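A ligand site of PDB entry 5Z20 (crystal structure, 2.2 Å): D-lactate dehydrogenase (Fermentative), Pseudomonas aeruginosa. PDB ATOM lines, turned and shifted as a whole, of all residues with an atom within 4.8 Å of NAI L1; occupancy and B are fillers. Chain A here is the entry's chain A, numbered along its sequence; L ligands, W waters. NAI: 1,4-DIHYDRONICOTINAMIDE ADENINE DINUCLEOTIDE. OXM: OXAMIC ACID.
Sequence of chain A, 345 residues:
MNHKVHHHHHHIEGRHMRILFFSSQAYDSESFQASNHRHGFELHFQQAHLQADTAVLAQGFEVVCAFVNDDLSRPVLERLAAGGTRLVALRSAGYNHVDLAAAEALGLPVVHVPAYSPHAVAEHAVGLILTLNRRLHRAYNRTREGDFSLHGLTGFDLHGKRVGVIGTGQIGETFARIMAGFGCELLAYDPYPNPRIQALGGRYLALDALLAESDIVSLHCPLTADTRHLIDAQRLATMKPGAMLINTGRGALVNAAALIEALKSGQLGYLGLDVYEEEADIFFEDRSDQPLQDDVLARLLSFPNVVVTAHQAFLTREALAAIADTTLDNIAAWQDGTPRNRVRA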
ATOM      1  N   ALA A  93     -24.973 -22.252  25.487  1.00  0.00           N
ATOM      2  CA  ALA A  93     -26.359 -22.302  25.037  1.00  0.00           C
ATOM      3  C   ALA A  93     -26.605 -23.612  24.343  1.00  0.00           C
ATOM      4  O   ALA A  93     -27.666 -24.236  24.509  1.00  0.00           O
ATOM      5  CB  ALA A  93     -26.633 -21.169  24.076  1.00  0.00           C
ATOM      6  N   GLY A  94     -25.655 -24.005  23.494  1.00  0.00           N
ATOM      7  CA  GLY A  94     -25.784 -25.229  22.717  1.00  0.00           C
ATOM      8  C   GLY A  94     -25.591 -26.496  23.501  1.00  0.00           C
ATOM      9  O   GLY A  94     -24.897 -26.500  24.506  1.00  0.00           O
ATOM     10  N   ASN A  96     -25.752 -29.910  21.560  1.00  0.00           N
ATOM     11  CA  ASN A  96     -25.655 -31.059  20.634  1.00  0.00           C
ATOM     12  C   ASN A  96     -24.611 -32.064  21.079  1.00  0.00           C
ATOM     13  O   ASN A  96     -24.533 -33.116  20.539  1.00  0.00           O
ATOM     14  CB  ASN A  96     -25.337 -30.570  19.214  1.00  0.00           C
ATOM     15  CG  ASN A  96     -24.099 -29.583  19.172  1.00  0.00           C
ATOM     16  OD1 ASN A  96     -24.213 -28.384  19.383  1.00  0.00           O
ATOM     17  ND2 ASN A  96     -22.933 -30.140  19.036  1.00  0.00           N
ATOM     18  N   PRO A 114     -29.349 -20.353  27.878  1.00  0.00           N
ATOM     19  CA  PRO A 114     -29.855 -20.176  26.578  1.00  0.00           C
ATOM     20  C   PRO A 114     -29.739 -18.798  26.009  1.00  0.00           C
ATOM     21  O   PRO A 114     -29.734 -18.677  24.765  1.00  0.00           O
ATOM     22  CB  PRO A 114     -31.375 -20.573  26.724  1.00  0.00           C
ATOM     23  CG  PRO A 114     -31.705 -20.223  28.133  1.00  0.00           C
ATOM     24  CD  PRO A 114     -30.432 -20.635  28.854  1.00  0.00           C
ATOM     25  N   TYR A 116     -27.329 -15.995  27.385  1.00  0.00           N
ATOM     26  CA  TYR A 116     -26.378 -15.121  28.010  1.00  0.00           C
ATOM     27  C   TYR A 116     -26.133 -13.836  27.249  1.00  0.00           C
ATOM     28  O   TYR A 116     -26.006 -12.810  27.891  1.00  0.00           O
ATOM     29  CB  TYR A 116     -25.074 -15.830  28.278  1.00  0.00           C
ATOM     30  CG  TYR A 116     -24.444 -16.530  27.159  1.00  0.00           C
ATOM     31  CD1 TYR A 116     -23.600 -15.845  26.287  1.00  0.00           C
ATOM     32  CD2 TYR A 116     -24.699 -17.848  26.898  1.00  0.00           C
ATOM     33  CE1 TYR A 116     -23.034 -16.517  25.199  1.00  0.00           C
ATOM     34  CE2 TYR A 116     -24.087 -18.521  25.827  1.00  0.00           C
ATOM     35  CZ  TYR A 116     -23.232 -17.857  25.027  1.00  0.00           C
ATOM     36  OH  TYR A 116     -22.667 -18.491  23.967  1.00  0.00           O
ATOM     37  N   VAL A 121     -22.682 -12.969  20.130  1.00  0.00           N
ATOM     38  CA  VAL A 121     -22.428 -13.902  19.039  1.00  0.00           C
ATOM     39  C   VAL A 121     -22.769 -13.237  17.674  1.00  0.00           C
ATOM     40  O   VAL A 121     -21.995 -13.331  16.713  1.00  0.00           O
ATOM     41  CB  VAL A 121     -23.267 -15.142  19.187  1.00  0.00           C
ATOM     42  CG1 VAL A 121     -22.960 -16.164  18.089  1.00  0.00           C
ATOM     43  CG2 VAL A 121     -23.023 -15.775  20.545  1.00  0.00           C
ATOM     44  N   ILE A 166     -30.037 -18.168   8.084  1.00  0.00           N
ATOM     45  CA  ILE A 166     -30.555 -19.510   8.241  1.00  0.00           C
ATOM     46  C   ILE A 166     -30.643 -19.823   9.735  1.00  0.00           C
ATOM     47  O   ILE A 166     -29.648 -19.896  10.407  1.00  0.00           O
ATOM     48  CB  ILE A 166     -29.606 -20.510   7.557  1.00  0.00           C
ATOM     49  CG1 ILE A 166     -29.669 -20.299   6.029  1.00  0.00           C
ATOM     50  CG2 ILE A 166     -29.986 -21.959   7.895  1.00  0.00           C
ATOM     51  CD1 ILE A 166     -28.642 -21.041   5.251  1.00  0.00           C
ATOM     52  N   GLY A 167     -31.881 -19.881  10.242  1.00  0.00           N
ATOM     53  CA  GLY A 167     -32.149 -19.902  11.645  1.00  0.00           C
ATOM     54  C   GLY A 167     -32.344 -18.534  12.249  1.00  0.00           C
ATOM     55  O   GLY A 167     -31.347 -17.833  12.573  1.00  0.00           O
ATOM     56  N   THR A 168     -33.596 -18.125  12.371  1.00  0.00           N
ATOM     57  CA  THR A 168     -33.978 -16.798  12.879  1.00  0.00           C
ATOM     58  C   THR A 168     -34.435 -16.890  14.347  1.00  0.00           C
ATOM     59  O   THR A 168     -35.467 -16.386  14.711  1.00  0.00           O
ATOM     60  CB  THR A 168     -35.052 -16.157  12.009  1.00  0.00           C
ATOM     61  OG1 THR A 168     -36.194 -17.012  11.845  1.00  0.00           O
ATOM     62  CG2 THR A 168     -34.489 -15.884  10.642  1.00  0.00           C
ATOM     63  N   GLY A 169     -33.608 -17.519  15.200  1.00  0.00           N
ATOM     64  CA  GLY A 169     -33.863 -17.639  16.619  1.00  0.00           C
ATOM     65  C   GLY A 169     -33.268 -16.444  17.352  1.00  0.00           C
ATOM     66  O   GLY A 169     -33.194 -15.361  16.827  1.00  0.00           O
ATOM     67  N   GLN A 170     -32.830 -16.637  18.566  1.00  0.00           N
ATOM     68  CA  GLN A 170     -32.357 -15.496  19.339  1.00  0.00           C
ATOM     69  C   GLN A 170     -31.144 -14.837  18.690  1.00  0.00           C
ATOM     70  O   GLN A 170     -31.112 -13.616  18.579  1.00  0.00           O
ATOM     71  CB  GLN A 170     -32.013 -15.938  20.748  1.00  0.00           C
ATOM     72  CG  GLN A 170     -33.295 -16.299  21.540  1.00  0.00           C
ATOM     73  CD  GLN A 170     -33.031 -17.056  22.826  1.00  0.00           C
ATOM     74  OE1 GLN A 170     -33.055 -16.465  23.909  1.00  0.00           O
ATOM     75  NE2 GLN A 170     -32.656 -18.327  22.706  1.00  0.00           N
ATOM     76  N   ILE A 171     -30.137 -15.642  18.300  1.00  0.00           N
ATOM     77  CA  ILE A 171     -28.955 -15.098  17.711  1.00  0.00           C
ATOM     78  C   ILE A 171     -29.227 -14.632  16.256  1.00  0.00           C
ATOM     79  O   ILE A 171     -28.909 -13.509  15.895  1.00  0.00           O
ATOM     80  CB  ILE A 171     -27.782 -16.069  17.745  1.00  0.00           C
ATOM     81  CG1 ILE A 171     -27.393 -16.313  19.206  1.00  0.00           C
ATOM     82  CG2 ILE A 171     -26.569 -15.466  17.009  1.00  0.00           C
ATOM     83  CD1 ILE A 171     -26.459 -17.501  19.390  1.00  0.00           C
ATOM     84  N   GLY A 172     -29.909 -15.455  15.491  1.00  0.00           N
ATOM     85  CA  GLY A 172     -30.203 -15.108  14.107  1.00  0.00           C
ATOM     86  C   GLY A 172     -30.975 -13.820  13.987  1.00  0.00           C
ATOM     87  O   GLY A 172     -30.739 -13.046  13.063  1.00  0.00           O
ATOM     88  N   TYR A 189     -34.704 -18.011   6.440  1.00  0.00           N
ATOM     89  CA  TYR A 189     -35.227 -19.337   6.386  1.00  0.00           C
ATOM     90  C   TYR A 189     -35.208 -19.981   7.737  1.00  0.00           C
ATOM     91  O   TYR A 189     -34.145 -19.976   8.420  1.00  0.00           O
ATOM     92  CB  TYR A 189     -34.354 -20.161   5.422  1.00  0.00           C
ATOM     93  CG  TYR A 189     -34.589 -21.614   5.521  1.00  0.00           C
ATOM     94  CD1 TYR A 189     -35.728 -22.192   4.925  1.00  0.00           C
ATOM     95  CD2 TYR A 189     -33.706 -22.442   6.214  1.00  0.00           C
ATOM     96  CE1 TYR A 189     -35.892 -23.560   5.004  1.00  0.00           C
ATOM     97  CE2 TYR A 189     -33.878 -23.805   6.303  1.00  0.00           C
ATOM     98  CZ  TYR A 189     -34.972 -24.344   5.662  1.00  0.00           C
ATOM     99  OH  TYR A 189     -35.098 -25.665   5.735  1.00  0.00           O
ATOM    100  N   ASP A 190     -36.350 -20.511   8.132  1.00  0.00           N
ATOM    101  CA  ASP A 190     -36.530 -21.116   9.432  1.00  0.00           C
ATOM    102  C   ASP A 190     -37.806 -21.987   9.377  1.00  0.00           C
ATOM    103  O   ASP A 190     -38.757 -21.598   8.761  1.00  0.00           O
ATOM    104  CB  ASP A 190     -36.745 -20.035  10.490  1.00  0.00           C
ATOM    105  CG  ASP A 190     -36.478 -20.512  11.926  1.00  0.00           C
ATOM    106  OD1 ASP A 190     -37.291 -21.296  12.471  1.00  0.00           O
ATOM    107  OD2 ASP A 190     -35.447 -20.139  12.513  1.00  0.00           O
ATOM    108  N   PRO A 191     -37.825 -23.120  10.054  1.00  0.00           N
ATOM    109  CA  PRO A 191     -39.109 -23.886  10.072  1.00  0.00           C
ATOM    110  C   PRO A 191     -40.179 -23.075  10.727  1.00  0.00           C
ATOM    111  O   PRO A 191     -41.326 -23.357  10.481  1.00  0.00           O
ATOM    112  CB  PRO A 191     -38.781 -25.142  10.928  1.00  0.00           C
ATOM    113  CG  PRO A 191     -37.514 -24.725  11.689  1.00  0.00           C
ATOM    114  CD  PRO A 191     -36.741 -23.821  10.746  1.00  0.00           C
ATOM    115  N   TYR A 192     -39.846 -22.058  11.527  1.00  0.00           N
ATOM    116  CA  TYR A 192     -40.861 -21.191  12.135  1.00  0.00           C
ATOM    117  C   TYR A 192     -40.848 -19.658  11.801  1.00  0.00           C
ATOM    118  O   TYR A 192     -39.898 -19.015  11.982  1.00  0.00           O
ATOM    119  CB  TYR A 192     -40.892 -21.405  13.669  1.00  0.00           C
ATOM    120  CG  TYR A 192     -41.131 -22.871  14.050  1.00  0.00           C
ATOM    121  CD1 TYR A 192     -42.377 -23.468  13.904  1.00  0.00           C
ATOM    122  CD2 TYR A 192     -40.083 -23.669  14.501  1.00  0.00           C
ATOM    123  CE1 TYR A 192     -42.587 -24.782  14.242  1.00  0.00           C
ATOM    124  CE2 TYR A 192     -40.260 -25.005  14.819  1.00  0.00           C
ATOM    125  CZ  TYR A 192     -41.533 -25.548  14.700  1.00  0.00           C
ATOM    126  OH  TYR A 192     -41.695 -26.859  15.006  1.00  0.00           O
ATOM    127  N   HIS A 220     -27.240 -19.720  11.793  1.00  0.00           N
ATOM    128  CA  HIS A 220     -27.592 -19.586  13.230  1.00  0.00           C
ATOM    129  C   HIS A 220     -28.643 -20.622  13.707  1.00  0.00           C
ATOM    130  O   HIS A 220     -29.377 -20.378  14.655  1.00  0.00           O
ATOM    131  CB  HIS A 220     -28.080 -18.157  13.465  1.00  0.00           C
ATOM    132  CG  HIS A 220     -27.050 -17.124  13.170  1.00  0.00           C
ATOM    133  ND1 HIS A 220     -25.930 -16.922  13.945  1.00  0.00           N
ATOM    134  CD2 HIS A 220     -26.928 -16.263  12.116  1.00  0.00           C
ATOM    135  CE1 HIS A 220     -25.177 -15.963  13.411  1.00  0.00           C
ATOM    136  NE2 HIS A 220     -25.757 -15.538  12.298  1.00  0.00           N
ATOM    137  N   CYS A 221     -28.704 -21.750  13.009  1.00  0.00           N
ATOM    138  CA  CYS A 221     -29.537 -22.847  13.448  1.00  0.00           C
ATOM    139  C   CYS A 221     -28.699 -23.740  14.369  1.00  0.00           C
ATOM    140  O   CYS A 221     -27.491 -23.803  14.204  1.00  0.00           O
ATOM    141  CB  CYS A 221     -30.039 -23.626  12.218  1.00  0.00           C
ATOM    142  SG  CYS A 221     -28.721 -24.154  11.096  1.00  0.00           S
ATOM    143  N   PRO A 222     -29.342 -24.518  15.236  1.00  0.00           N
ATOM    144  CA  PRO A 222     -28.590 -25.517  16.019  1.00  0.00           C
ATOM    145  C   PRO A 222     -28.160 -26.652  15.173  1.00  0.00           C
ATOM    146  O   PRO A 222     -28.668 -26.842  14.011  1.00  0.00           O
ATOM    147  CB  PRO A 222     -29.573 -25.967  17.041  1.00  0.00           C
ATOM    148  CG  PRO A 222     -30.918 -25.584  16.528  1.00  0.00           C
ATOM    149  CD  PRO A 222     -30.767 -24.553  15.490  1.00  0.00           C
ATOM    150  N   LEU A 223     -27.218 -27.393  15.696  1.00  0.00           N
ATOM    151  CA  LEU A 223     -26.800 -28.675  15.042  1.00  0.00           C
ATOM    152  C   LEU A 223     -27.758 -29.789  15.519  1.00  0.00           C
ATOM    153  O   LEU A 223     -27.905 -29.995  16.718  1.00  0.00           O
ATOM    154  CB  LEU A 223     -25.358 -29.026  15.397  1.00  0.00           C
ATOM    155  CG  LEU A 223     -24.882 -30.389  14.847  1.00  0.00           C
ATOM    156  CD1 LEU A 223     -24.970 -30.382  13.345  1.00  0.00           C
ATOM    157  CD2 LEU A 223     -23.496 -30.740  15.336  1.00  0.00           C
ATOM    158  N   ASP A 226     -31.066 -32.955  11.289  1.00  0.00           N
ATOM    159  CA  ASP A 226     -31.507 -32.286  10.070  1.00  0.00           C
ATOM    160  C   ASP A 226     -30.634 -31.139   9.565  1.00  0.00           C
ATOM    161  O   ASP A 226     -30.807 -30.729   8.450  1.00  0.00           O
ATOM    162  CB  ASP A 226     -32.853 -31.663  10.292  1.00  0.00           C
ATOM    163  CG  ASP A 226     -33.907 -32.700  10.639  1.00  0.00           C
ATOM    164  OD1 ASP A 226     -33.820 -33.898  10.189  1.00  0.00           O
ATOM    165  OD2 ASP A 226     -34.822 -32.304  11.385  1.00  0.00           O
ATOM    166  N   THR A 227     -29.743 -30.594  10.358  1.00  0.00           N
ATOM    167  CA  THR A 227     -28.902 -29.484   9.878  1.00  0.00           C
ATOM    168  C   THR A 227     -27.490 -29.931   9.599  1.00  0.00           C
ATOM    169  O   THR A 227     -26.656 -29.152   9.123  1.00  0.00           O
ATOM    170  CB  THR A 227     -28.902 -28.309  10.907  1.00  0.00           C
ATOM    171  OG1 THR A 227     -28.433 -28.770  12.169  1.00  0.00           O
ATOM    172  CG2 THR A 227     -30.255 -27.795  11.047  1.00  0.00           C
ATOM    173  N   THR A 248     -20.985 -19.220  12.515  1.00  0.00           N
ATOM    174  CA  THR A 248     -20.758 -19.084  13.939  1.00  0.00           C
ATOM    175  C   THR A 248     -21.719 -19.990  14.712  1.00  0.00           C
ATOM    176  O   THR A 248     -21.994 -19.756  15.876  1.00  0.00           O
ATOM    177  CB  THR A 248     -21.009 -17.649  14.421  1.00  0.00           C
ATOM    178  OG1 THR A 248     -22.355 -17.233  14.106  1.00  0.00           O
ATOM    179  CG2 THR A 248     -20.007 -16.675  13.750  1.00  0.00           C
ATOM    180  N   GLY A 249     -22.270 -21.008  14.034  1.00  0.00           N
ATOM    181  CA  GLY A 249     -23.171 -22.005  14.600  1.00  0.00           C
ATOM    182  C   GLY A 249     -22.440 -23.176  15.166  1.00  0.00           C
ATOM    183  O   GLY A 249     -22.013 -23.147  16.345  1.00  0.00           O
ATOM    184  N   ARG A 250     -22.227 -24.186  14.334  1.00  0.00           N
ATOM    185  CA  ARG A 250     -21.451 -25.354  14.736  1.00  0.00           C
ATOM    186  C   ARG A 250     -20.717 -25.891  13.538  1.00  0.00           C
ATOM    187  O   ARG A 250     -21.174 -25.773  12.391  1.00  0.00           O
ATOM    188  CB  ARG A 250     -22.337 -26.504  15.252  1.00  0.00           C
ATOM    189  CG  ARG A 250     -22.900 -26.318  16.697  1.00  0.00           C
ATOM    190  CD  ARG A 250     -21.836 -26.460  17.741  1.00  0.00           C
ATOM    191  NE  ARG A 250     -22.277 -26.281  19.119  1.00  0.00           N
ATOM    192  CZ  ARG A 250     -22.289 -25.096  19.746  1.00  0.00           C
ATOM    193  NH1 ARG A 250     -21.913 -23.986  19.142  1.00  0.00           N
ATOM    194  NH2 ARG A 250     -22.647 -25.009  21.036  1.00  0.00           N
ATOM    195  N   ASP A 274     -16.195 -19.431  12.900  1.00  0.00           N
ATOM    196  CA  ASP A 274     -15.859 -19.426  14.327  1.00  0.00           C
ATOM    197  C   ASP A 274     -15.892 -20.819  14.892  1.00  0.00           C
ATOM    198  O   ASP A 274     -15.587 -21.022  16.055  1.00  0.00           O
ATOM    199  CB  ASP A 274     -16.821 -18.551  15.081  1.00  0.00           C
ATOM    200  CG  ASP A 274     -16.413 -18.342  16.539  1.00  0.00           C
ATOM    201  OD1 ASP A 274     -15.245 -17.882  16.720  1.00  0.00           O
ATOM    202  OD2 ASP A 274     -17.255 -18.605  17.470  1.00  0.00           O
ATOM    203  N   VAL A 275     -16.268 -21.792  14.051  1.00  0.00           N
ATOM    204  CA  VAL A 275     -16.442 -23.165  14.462  1.00  0.00           C
ATOM    205  C   VAL A 275     -16.019 -24.105  13.351  1.00  0.00           C
ATOM    206  O   VAL A 275     -15.910 -23.725  12.173  1.00  0.00           O
ATOM    207  CB  VAL A 275     -17.908 -23.494  14.780  1.00  0.00           C
ATOM    208  CG1 VAL A 275     -18.302 -22.686  16.009  1.00  0.00           C
ATOM    209  CG2 VAL A 275     -18.839 -23.197  13.627  1.00  0.00           C
ATOM    210  N   HIS A 311     -13.669 -20.326  17.943  1.00  0.00           N
ATOM    211  CA  HIS A 311     -14.862 -20.435  18.752  1.00  0.00           C
ATOM    212  C   HIS A 311     -14.930 -19.420  19.877  1.00  0.00           C
ATOM    213  O   HIS A 311     -15.033 -19.770  21.054  1.00  0.00           O
ATOM    214  CB  HIS A 311     -14.986 -21.846  19.304  1.00  0.00           C
ATOM    215  CG  HIS A 311     -16.387 -22.261  19.595  1.00  0.00           C
ATOM    216  ND1 HIS A 311     -16.853 -23.524  19.362  1.00  0.00           N
ATOM    217  CD2 HIS A 311     -17.436 -21.551  20.065  1.00  0.00           C
ATOM    218  CE1 HIS A 311     -18.131 -23.608  19.722  1.00  0.00           C
ATOM    219  NE2 HIS A 311     -18.501 -22.421  20.179  1.00  0.00           N
ATOM    220  N   ALA A 313     -16.905 -16.547  19.449  1.00  0.00           N
ATOM    221  CA  ALA A 313     -18.092 -15.680  19.333  1.00  0.00           C
ATOM    222  C   ALA A 313     -18.817 -15.370  20.627  1.00  0.00           C
ATOM    223  O   ALA A 313     -19.374 -14.257  20.779  1.00  0.00           O
ATOM    224  CB  ALA A 313     -19.080 -16.246  18.356  1.00  0.00           C
ATOM    225  N   PHE A 314     -18.728 -16.281  21.592  1.00  0.00           N
ATOM    226  CA  PHE A 314     -19.334 -16.085  22.888  1.00  0.00           C
ATOM    227  C   PHE A 314     -18.484 -15.214  23.801  1.00  0.00           C
ATOM    228  O   PHE A 314     -18.921 -14.839  24.873  1.00  0.00           O
ATOM    229  CB  PHE A 314     -19.559 -17.456  23.593  1.00  0.00           C
ATOM    230  CG  PHE A 314     -18.293 -18.057  24.137  1.00  0.00           C
ATOM    231  CD1 PHE A 314     -17.414 -18.752  23.325  1.00  0.00           C
ATOM    232  CD2 PHE A 314     -17.974 -17.938  25.456  1.00  0.00           C
ATOM    233  CE1 PHE A 314     -16.206 -19.254  23.825  1.00  0.00           C
ATOM    234  CE2 PHE A 314     -16.800 -18.478  25.971  1.00  0.00           C
ATOM    235  CZ  PHE A 314     -15.904 -19.104  25.142  1.00  0.00           C
HETATM  236  PA  NAI L   1     -32.398 -20.513  19.316  1.00  0.00           P
HETATM  237  O1A NAI L   1     -32.928 -21.743  19.697  1.00  0.00           O
HETATM  238  O2A NAI L   1     -32.880 -19.342  19.881  1.00  0.00           O
HETATM  239  O5B NAI L   1     -32.748 -20.341  17.827  1.00  0.00           O
HETATM  240  C5B NAI L   1     -32.599 -21.360  16.888  1.00  0.00           C
HETATM  241  C4B NAI L   1     -33.406 -21.145  15.633  1.00  0.00           C
HETATM  242  O4B NAI L   1     -32.987 -22.076  14.683  1.00  0.00           O
HETATM  243  C3B NAI L   1     -34.889 -21.361  15.824  1.00  0.00           C
HETATM  244  O3B NAI L   1     -35.576 -20.313  15.204  1.00  0.00           O
HETATM  245  C2B NAI L   1     -35.192 -22.650  15.132  1.00  0.00           C
HETATM  246  O2B NAI L   1     -36.478 -22.663  14.593  1.00  0.00           O
HETATM  247  C1B NAI L   1     -34.120 -22.624  14.084  1.00  0.00           C
HETATM  248  N9A NAI L   1     -33.971 -23.952  13.500  1.00  0.00           N
HETATM  249  C8A NAI L   1     -34.087 -25.092  14.142  1.00  0.00           C
HETATM  250  N7A NAI L   1     -33.939 -26.096  13.333  1.00  0.00           N
HETATM  251  C5A NAI L   1     -33.734 -25.609  12.151  1.00  0.00           C
HETATM  252  C6A NAI L   1     -33.508 -26.144  10.841  1.00  0.00           C
HETATM  253  N6A NAI L   1     -33.489 -27.409  10.701  1.00  0.00           N
HETATM  254  N1A NAI L   1     -33.327 -25.324   9.827  1.00  0.00           N
HETATM  255  C2A NAI L   1     -33.352 -24.029  10.005  1.00  0.00           C
HETATM  256  N3A NAI L   1     -33.562 -23.483  11.173  1.00  0.00           N
HETATM  257  C4A NAI L   1     -33.760 -24.194  12.250  1.00  0.00           C
HETATM  258  O3  NAI L   1     -30.855 -20.563  19.452  1.00  0.00           O
HETATM  259  PN  NAI L   1     -29.795 -19.443  19.371  1.00  0.00           P
HETATM  260  O1N NAI L   1     -29.621 -19.056  20.698  1.00  0.00           O
HETATM  261  O2N NAI L   1     -30.083 -18.494  18.344  1.00  0.00           O
HETATM  262  O5D NAI L   1     -28.643 -20.402  19.084  1.00  0.00           O
HETATM  263  C5D NAI L   1     -28.241 -20.813  17.815  1.00  0.00           C
HETATM  264  C4D NAI L   1     -27.033 -21.720  17.782  1.00  0.00           C
HETATM  265  O4D NAI L   1     -25.837 -20.986  17.751  1.00  0.00           O
HETATM  266  C3D NAI L   1     -26.884 -22.714  18.941  1.00  0.00           C
HETATM  267  O3D NAI L   1     -27.590 -23.892  18.746  1.00  0.00           O
HETATM  268  C2D NAI L   1     -25.401 -22.925  18.982  1.00  0.00           C
HETATM  269  O2D NAI L   1     -25.045 -24.072  18.282  1.00  0.00           O
HETATM  270  C1D NAI L   1     -24.803 -21.748  18.250  1.00  0.00           C
HETATM  271  N1N NAI L   1     -24.003 -20.944  19.140  1.00  0.00           N
HETATM  272  C2N NAI L   1     -22.735 -20.719  18.850  1.00  0.00           C
HETATM  273  C3N NAI L   1     -21.913 -19.935  19.660  1.00  0.00           C
HETATM  274  C7N NAI L   1     -20.472 -19.649  19.356  1.00  0.00           C
HETATM  275  O7N NAI L   1     -19.752 -19.345  20.227  1.00  0.00           O
HETATM  276  N7N NAI L   1     -19.992 -19.647  18.154  1.00  0.00           N
HETATM  277  C4N NAI L   1     -22.463 -19.417  20.809  1.00  0.00           C
HETATM  278  C5N NAI L   1     -23.779 -19.664  21.072  1.00  0.00           C
HETATM  279  C6N NAI L   1     -24.547 -20.435  20.228  1.00  0.00           C
HETATM  280  C1  OXM L   2     -21.272 -21.759  22.438  1.00  0.00           C
HETATM  281  N1  OXM L   2     -20.381 -20.928  22.989  1.00  0.00           N
HETATM  282  O1  OXM L   2     -21.052 -22.332  21.393  1.00  0.00           O
HETATM  283  C2  OXM L   2     -22.541 -21.976  23.129  1.00  0.00           C
HETATM  284  O2  OXM L   2     -23.228 -22.980  22.829  1.00  0.00           O
HETATM  285  O3  OXM L   2     -22.917 -21.149  23.984  1.00  0.00           O
HETATM  286  O   HOH W   1     -34.355 -25.125  17.524  1.00  0.00           O
HETATM  287  O   HOH W   2     -26.173 -26.694  18.467  1.00  0.00           O
HETATM  288  O   HOH W   3     -24.962 -18.840  15.958  1.00  0.00           O
HETATM  289  O   HOH W   4     -32.971 -26.728   7.469  1.00  0.00           O
HETATM  290  O   HOH W   5     -25.178 -24.163  15.274  1.00  0.00           O
HETATM  291  O   HOH W   6     -32.852 -21.629  22.617  1.00  0.00           O
HETATM  292  O   HOH W   7     -30.138 -20.691  22.906  1.00  0.00           O
HETATM  293  O   HOH W   8     -33.307 -29.479   8.432  1.00  0.00           O
HETATM  294  O   HOH W   9     -35.251 -23.057  19.172  1.00  0.00           O
HETATM  295  O   HOH W  10     -33.362 -29.538  13.169  1.00  0.00           O
HETATM  296  O   HOH W  11     -29.467 -24.738  20.702  1.00  0.00           O
HETATM  297  O   HOH W  12     -30.860 -18.232  15.728  1.00  0.00           O
HETATM  298  O   HOH W  13     -32.011 -24.332  19.472  1.00  0.00           O
HETATM  299  O   HOH W  14     -28.818 -17.293  22.673  1.00  0.00           O
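Water W12 lies within hydrogen-bond range of O2N of NAI L1, O of His 220, N of Gly 169, N of Gly 172 and O of Gly 167.
Water W14 bridges the backbone carbonyl oxygen (O) of Pro 114 and an oxygen (O1N) of NAI L1.
Water W4 bridges a nitrogen (N1A) of NAI L1 (2.8 Å) and the side-chain hydroxyl of Tyr 189 (2.9 Å).
Water W2 lies within hydrogen-bond range of OD1 of Asn 96 (2.7 Å), O2D of NAI L1 (2.9 Å) and N of Leu 223 (3.0 Å).
Water W3 lies within hydrogen-bond range of an oxygen (O4D) of NAI L1 (2.9 Å), a ring nitrogen (ND1) of His 220 (2.9 Å) and the backbone carbonyl oxygen (O) of Thr 248 (3.1 Å).
Water W8 bridges the backbone carbonyl oxygen (O) of Asp 226 (2.8 Å) and a nitrogen (N6A) of NAI L1 (3.1 Å).
Residues that only touch NAI L1: Tyr 116 (3.3 Å), Val 121 (3.7 Å), Gly 167 (3.8 Å), Thr 168 (3.7 Å), Tyr 189 (3.7 Å), Pro 191 (3.2 Å), Tyr 192 (3.7 Å), His 220 (3.4 Å), Cys 221 (3.7 Å), Pro 222 (3.3 Å), Thr 227 (3.3 Å), Gly 249 (3.6 Å), Ala 313 (3.5 Å) and Phe 314 (3.5 Å).
Hydrophobic or aromatic side chains within 4 Å of NAI L1: Val 121, Ile 171, Tyr 189, Pro 191, Tyr 192, Pro 222, His 311, Ala 313 and Phe 314.
Within 4 Å of NAI L1: Tyr 116, Val 121, Gly 167, Thr 168, Gly 169, Gln 170, Ile 171, Tyr 189, Asp 190, Pro 191, Tyr 192, His 220, Cys 221, Pro 222, Thr 227, Thr 248, Gly 249, Arg 250, Asp 274, His 311, Ala 313 and Phe 314.
NH1 of Arg 250 lies within hydrogen-bond range of O2D of NAI L1.
A nitrogen (N7N) of NAI L1 lies within hydrogen-bond range of the backbone carbonyl oxygen of Thr 248, 3.0 Å away.
NE2 of Gln 170 sits at hydrogen-bond distance from O2A of NAI L1 (3.0 Å).
A ring nitrogen (NE2) of His 311 is in hydrogen-bond range of an oxygen (O1) of OXM L2 (2.8 Å).
O3 of OXM L2 is in hydrogen-bond range of N of Ala 93, 2.8 Å away.
The side-chain carboxylate (OD1) of Asp 190 lies within hydrogen-bond range of an oxygen (O2B) of NAI L1 (2.7 Å).
The guanidinium group of Arg 250 lies within salt-bridge range of an oxygen (O2) of OXM L2 (2.8 Å).
The side-chain carboxylate (OD2) of Asp 274 sits at hydrogen-bond distance from a nitrogen (N7N) of NAI L1 (3.0 Å).
The backbone NH (N) of Gly 94 sits at hydrogen-bond distance from an oxygen (O2) of OXM L2, 2.7 Å away.
The backbone NH (N) of Gly 169 lies within hydrogen-bond range of an oxygen (O3B) of NAI L1, at 3.4 Å.
An oxygen (O7N) of NAI L1 lies close to a ring nitrogen (NE2) of His 311 (3.3 Å).
The side-chain hydroxyl (OH) of Tyr 116 is in hydrogen-bond range of an oxygen (O3) of OXM L2 (2.7 Å).
The backbone NH (N) of Ile 171 is in hydrogen-bond range of an oxygen (O2N) of NAI L1 (2.9 Å).
The backbone NH (N) of Gln 170 is in hydrogen-bond range of an oxygen (O2A) of NAI L1 (3.0 Å).
O7N of NAI L1 is in hydrogen-bond range of N1 of OXM L2 (3.2 Å).
OD2 of Asp 190 sits at hydrogen-bond distance from N of Thr 168 (2.7 Å).
The backbone NH (N) of His 220 lies within hydrogen-bond range of the backbone carbonyl oxygen (O) of Ile 166.
The side-chain hydroxyl (OG1) of Thr 227 is in hydrogen-bond range of the backbone carbonyl oxygen (O) of Pro 222 (2.7 Å).
The backbone NH of Ala 313 is in hydrogen-bond range of the side-chain carboxylate of Asp 274, 2.9 Å away.
O of Tyr 189 sits at hydrogen-bond distance from N of Gly 167.
N of Cys 221 sits at hydrogen-bond distance from O of Ile 166.
O of Asp 274 sits at hydrogen-bond distance from N of His 311 (2.8 Å).
The side-chain amide oxygen (OD1) of Asn 96 sits at hydrogen-bond distance from the guanidinium group (NE) of Arg 250 (2.9 Å).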
